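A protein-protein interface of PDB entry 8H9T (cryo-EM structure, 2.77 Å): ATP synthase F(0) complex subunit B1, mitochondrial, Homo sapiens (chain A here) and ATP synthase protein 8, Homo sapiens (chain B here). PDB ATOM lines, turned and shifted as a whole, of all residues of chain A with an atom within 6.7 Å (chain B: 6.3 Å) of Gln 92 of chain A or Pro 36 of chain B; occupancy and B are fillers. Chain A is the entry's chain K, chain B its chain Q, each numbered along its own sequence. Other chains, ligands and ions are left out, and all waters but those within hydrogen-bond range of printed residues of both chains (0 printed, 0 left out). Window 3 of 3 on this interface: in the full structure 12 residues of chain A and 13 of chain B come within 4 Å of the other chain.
His 34 of chain B touches Lys 89 of chain A (NE2 to CE, 3.3 Å). NE2 of Gln 92 of chain A touches CB of Pro 36 of chain B, at 3.6 Å. Gln 92 of chain A touches Pro 37 of chain B. Pro 37 of chain B touches Leu 93 of chain A. Ala 96 of chain A touches Pro 37 of chain B (CB to CB, 3.6 Å). Ala 96 of chain A touches Pro 39 of chain B (O to CB, 3.1 Å).
Of the printed residues of chain B, Lys 89 of chain A touches His 34. Leu 90 of chain A touches none of the printed residues of chain B. Gln 92 of chain A touches two residues of chain B. Printed residues of chain B within 4 Å of Ala 96 of chain A: Pro 37 and Pro 39. Pro 36 of chain B touches just one residue of chain A: Gln 92. Of the printed residues of chain A, Pro 39 of chain B touches Ala 96. The nearest residue of chain B that does not touch Gln 92 of chain A is His 34 of chain B (6.2 Å). The nearest printed residue of chain B that does not touch Leu 93 of chain A is His 34 of chain B (5.1 Å).
Printed residues of chain B that touch a printed residue of chain A: His 34, Pro 36, Pro 37 and Pro 39. Hydrophobic or aromatic side chains of chain B that line the printed part of chain A: His 34, Pro 36, Pro 37 and Pro 39. Among the printed residues, 6 pairs touch across the chains. Among the printed residues, no Asp or Glu carboxylate lies within 4 Å of a Lys or Arg side-chain nitrogen of the other chain.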
ATOM      1  N   GLU A  87      23.607 -11.055  24.523  1.00  0.00           N
ATOM      2  CA  GLU A  87      24.471 -11.281  23.370  1.00  0.00           C
ATOM      3  C   GLU A  87      25.073 -12.675  23.398  1.00  0.00           C
ATOM      4  O   GLU A  87      25.197 -13.322  22.355  1.00  0.00           O
ATOM      5  CB  GLU A  87      25.577 -10.232  23.310  1.00  0.00           C
ATOM      6  CG  GLU A  87      25.074  -8.807  23.221  1.00  0.00           C
ATOM      7  CD  GLU A  87      23.886  -8.665  22.297  1.00  0.00           C
ATOM      8  OE1 GLU A  87      23.978  -9.106  21.134  1.00  0.00           O
ATOM      9  OE2 GLU A  87      22.857  -8.113  22.735  1.00  0.00           O
ATOM     10  N   GLN A  88      25.460 -13.153  24.577  1.00  0.00           N
ATOM     11  CA  GLN A  88      25.997 -14.502  24.670  1.00  0.00           C
ATOM     12  C   GLN A  88      24.951 -15.532  24.280  1.00  0.00           C
ATOM     13  O   GLN A  88      25.249 -16.474  23.540  1.00  0.00           O
ATOM     14  CB  GLN A  88      26.515 -14.769  26.077  1.00  0.00           C
ATOM     15  CG  GLN A  88      27.873 -14.165  26.347  1.00  0.00           C
ATOM     16  CD  GLN A  88      28.436 -14.590  27.683  1.00  0.00           C
ATOM     17  OE1 GLN A  88      29.509 -14.147  28.087  1.00  0.00           O
ATOM     18  NE2 GLN A  88      27.713 -15.456  28.379  1.00  0.00           N
ATOM     19  N   LYS A  89      23.717 -15.370  24.760  1.00  0.00           N
ATOM     20  CA  LYS A  89      22.672 -16.310  24.367  1.00  0.00           C
ATOM     21  C   LYS A  89      22.460 -16.294  22.860  1.00  0.00           C
ATOM     22  O   LYS A  89      22.341 -17.351  22.225  1.00  0.00           O
ATOM     23  CB  LYS A  89      21.373 -15.982  25.087  1.00  0.00           C
ATOM     24  CG  LYS A  89      20.269 -16.970  24.821  1.00  0.00           C
ATOM     25  CD  LYS A  89      19.124 -16.754  25.788  1.00  0.00           C
ATOM     26  CE  LYS A  89      18.631 -18.069  26.352  1.00  0.00           C
ATOM     27  NZ  LYS A  89      17.801 -17.872  27.567  1.00  0.00           N
ATOM     28  N   LEU A  90      22.430 -15.102  22.267  1.00  0.00           N
ATOM     29  CA  LEU A  90      22.201 -14.989  20.830  1.00  0.00           C
ATOM     30  C   LEU A  90      23.313 -15.666  20.041  1.00  0.00           C
ATOM     31  O   LEU A  90      23.054 -16.465  19.131  1.00  0.00           O
ATOM     32  CB  LEU A  90      22.093 -13.518  20.444  1.00  0.00           C
ATOM     33  CG  LEU A  90      21.507 -13.229  19.072  1.00  0.00           C
ATOM     34  CD1 LEU A  90      20.185 -13.933  18.952  1.00  0.00           C
ATOM     35  CD2 LEU A  90      21.333 -11.742  18.888  1.00  0.00           C
ATOM     36  N   ALA A  91      24.563 -15.349  20.373  1.00  0.00           N
ATOM     37  CA  ALA A  91      25.686 -15.924  19.647  1.00  0.00           C
ATOM     38  C   ALA A  91      25.734 -17.432  19.815  1.00  0.00           C
ATOM     39  O   ALA A  91      26.066 -18.157  18.871  1.00  0.00           O
ATOM     40  CB  ALA A  91      26.993 -15.292  20.114  1.00  0.00           C
ATOM     41  N   GLN A  92      25.413 -17.928  21.010  1.00  0.00           N
ATOM     42  CA  GLN A  92      25.377 -19.369  21.205  1.00  0.00           C
ATOM     43  C   GLN A  92      24.336 -20.010  20.305  1.00  0.00           C
ATOM     44  O   GLN A  92      24.598 -21.039  19.676  1.00  0.00           O
ATOM     45  CB  GLN A  92      25.099 -19.694  22.665  1.00  0.00           C
ATOM     46  CG  GLN A  92      24.612 -21.100  22.892  1.00  0.00           C
ATOM     47  CD  GLN A  92      24.332 -21.378  24.351  1.00  0.00           C
ATOM     48  OE1 GLN A  92      24.441 -20.492  25.194  1.00  0.00           O
ATOM     49  NE2 GLN A  92      23.966 -22.616  24.659  1.00  0.00           N
ATOM     50  N   LEU A  93      23.159 -19.399  20.196  1.00  0.00           N
ATOM     51  CA  LEU A  93      22.134 -19.979  19.333  1.00  0.00           C
ATOM     52  C   LEU A  93      22.550 -19.943  17.867  1.00  0.00           C
ATOM     53  O   LEU A  93      22.238 -20.861  17.099  1.00  0.00           O
ATOM     54  CB  LEU A  93      20.811 -19.255  19.533  1.00  0.00           C
ATOM     55  CG  LEU A  93      20.069 -19.694  20.786  1.00  0.00           C
ATOM     56  CD1 LEU A  93      19.163 -18.585  21.249  1.00  0.00           C
ATOM     57  CD2 LEU A  93      19.283 -20.951  20.514  1.00  0.00           C
ATOM     58  N   GLU A  94      23.262 -18.900  17.452  1.00  0.00           N
ATOM     59  CA  GLU A  94      23.650 -18.836  16.045  1.00  0.00           C
ATOM     60  C   GLU A  94      24.734 -19.855  15.721  1.00  0.00           C
ATOM     61  O   GLU A  94      24.672 -20.536  14.686  1.00  0.00           O
ATOM     62  CB  GLU A  94      24.102 -17.427  15.690  1.00  0.00           C
ATOM     63  CG  GLU A  94      22.939 -16.487  15.518  1.00  0.00           C
ATOM     64  CD  GLU A  94      23.267 -15.327  14.624  1.00  0.00           C
ATOM     65  OE1 GLU A  94      23.151 -14.172  15.083  1.00  0.00           O
ATOM     66  OE2 GLU A  94      23.644 -15.570  13.459  1.00  0.00           O
ATOM     67  N   GLU A  95      25.739 -19.972  16.589  1.00  0.00           N
ATOM     68  CA  GLU A  95      26.719 -21.033  16.431  1.00  0.00           C
ATOM     69  C   GLU A  95      26.104 -22.401  16.651  1.00  0.00           C
ATOM     70  O   GLU A  95      26.760 -23.413  16.401  1.00  0.00           O
ATOM     71  CB  GLU A  95      27.886 -20.831  17.392  1.00  0.00           C
ATOM     72  CG  GLU A  95      28.553 -19.479  17.272  1.00  0.00           C
ATOM     73  CD  GLU A  95      29.698 -19.315  18.244  1.00  0.00           C
ATOM     74  OE1 GLU A  95      30.524 -20.243  18.351  1.00  0.00           O
ATOM     75  OE2 GLU A  95      29.773 -18.259  18.904  1.00  0.00           O
ATOM     76  N   ALA A  96      24.876 -22.454  17.144  1.00  0.00           N
ATOM     77  CA  ALA A  96      24.141 -23.701  17.199  1.00  0.00           C
ATOM     78  C   ALA A  96      23.311 -23.952  15.954  1.00  0.00           C
ATOM     79  O   ALA A  96      22.884 -25.086  15.729  1.00  0.00           O
ATOM     80  CB  ALA A  96      23.232 -23.713  18.418  1.00  0.00           C
ATOM     81  N   LYS A  97      23.028 -22.918  15.177  1.00  0.00           N
ATOM     82  CA  LYS A  97      22.421 -23.124  13.867  1.00  0.00           C
ATOM     83  C   LYS A  97      23.445 -23.568  12.831  1.00  0.00           C
ATOM     84  O   LYS A  97      23.201 -24.512  12.060  1.00  0.00           O
ATOM     85  CB  LYS A  97      21.746 -21.840  13.391  1.00  0.00           C
ATOM     86  CG  LYS A  97      21.171 -21.944  12.006  1.00  0.00           C
ATOM     87  CD  LYS A  97      20.611 -20.621  11.555  1.00  0.00           C
ATOM     88  CE  LYS A  97      19.316 -20.323  12.263  1.00  0.00           C
ATOM     89  NZ  LYS A  97      18.667 -19.109  11.711  1.00  0.00           N
ATOM     90  N   HIS B  34      14.966 -23.317  28.791  1.00  0.00           N
ATOM     91  CA  HIS B  34      15.149 -24.322  27.757  1.00  0.00           C
ATOM     92  C   HIS B  34      16.553 -24.904  27.823  1.00  0.00           C
ATOM     93  O   HIS B  34      17.520 -24.194  28.110  1.00  0.00           O
ATOM     94  CB  HIS B  34      14.914 -23.702  26.389  1.00  0.00           C
ATOM     95  CG  HIS B  34      15.933 -22.675  26.026  1.00  0.00           C
ATOM     96  ND1 HIS B  34      17.201 -23.006  25.604  1.00  0.00           N
ATOM     97  CD2 HIS B  34      15.881 -21.326  26.042  1.00  0.00           C
ATOM     98  CE1 HIS B  34      17.883 -21.902  25.365  1.00  0.00           C
ATOM     99  NE2 HIS B  34      17.104 -20.868  25.621  1.00  0.00           N
ATOM    100  N   LEU B  35      16.661 -26.199  27.550  1.00  0.00           N
ATOM    101  CA  LEU B  35      17.965 -26.837  27.517  1.00  0.00           C
ATOM    102  C   LEU B  35      18.791 -26.252  26.377  1.00  0.00           C
ATOM    103  O   LEU B  35      18.240 -25.910  25.330  1.00  0.00           O
ATOM    104  CB  LEU B  35      17.821 -28.340  27.341  1.00  0.00           C
ATOM    105  CG  LEU B  35      16.977 -29.000  28.424  1.00  0.00           C
ATOM    106  CD1 LEU B  35      15.560 -29.177  27.946  1.00  0.00           C
ATOM    107  CD2 LEU B  35      17.566 -30.332  28.818  1.00  0.00           C
ATOM    108  N   PRO B  36      20.099 -26.119  26.548  1.00  0.00           N
ATOM    109  CA  PRO B  36      20.911 -25.433  25.548  1.00  0.00           C
ATOM    110  C   PRO B  36      20.868 -26.168  24.224  1.00  0.00           C
ATOM    111  O   PRO B  36      20.725 -27.398  24.193  1.00  0.00           O
ATOM    112  CB  PRO B  36      22.322 -25.464  26.150  1.00  0.00           C
ATOM    113  CG  PRO B  36      22.127 -25.770  27.585  1.00  0.00           C
ATOM    114  CD  PRO B  36      20.914 -26.628  27.658  1.00  0.00           C
ATOM    115  N   PRO B  37      20.982 -25.452  23.107  1.00  0.00           N
ATOM    116  CA  PRO B  37      21.000 -26.120  21.802  1.00  0.00           C
ATOM    117  C   PRO B  37      22.289 -26.912  21.657  1.00  0.00           C
ATOM    118  O   PRO B  37      23.385 -26.354  21.709  1.00  0.00           O
ATOM    119  CB  PRO B  37      20.922 -24.959  20.809  1.00  0.00           C
ATOM    120  CG  PRO B  37      21.503 -23.819  21.531  1.00  0.00           C
ATOM    121  CD  PRO B  37      21.234 -24.009  22.993  1.00  0.00           C
ATOM    122  N   SER B  38      22.165 -28.232  21.502  1.00  0.00           N
ATOM    123  CA  SER B  38      23.364 -29.086  21.289  1.00  0.00           C
ATOM    124  C   SER B  38      23.380 -29.597  19.843  1.00  0.00           C
ATOM    125  O   SER B  38      23.118 -30.799  19.640  1.00  0.00           O
ATOM    126  CB  SER B  38      23.396 -30.224  22.274  1.00  0.00           C
ATOM    127  OG  SER B  38      24.518 -31.063  22.040  1.00  0.00           O
ATOM    128  N   PRO B  39      23.674 -28.747  18.834  1.00  0.00           N
ATOM    129  CA  PRO B  39      23.644 -29.168  17.432  1.00  0.00           C
ATOM    130  C   PRO B  39      24.773 -30.168  17.154  1.00  0.00           C
ATOM    131  O   PRO B  39      25.852 -29.728  16.814  1.00  0.00           O
ATOM    132  CB  PRO B  39      23.885 -27.867  16.656  1.00  0.00           C
ATOM    133  CG  PRO B  39      24.661 -27.006  17.626  1.00  0.00           C
ATOM    134  CD  PRO B  39      24.082 -27.348  18.983  1.00  0.00           C
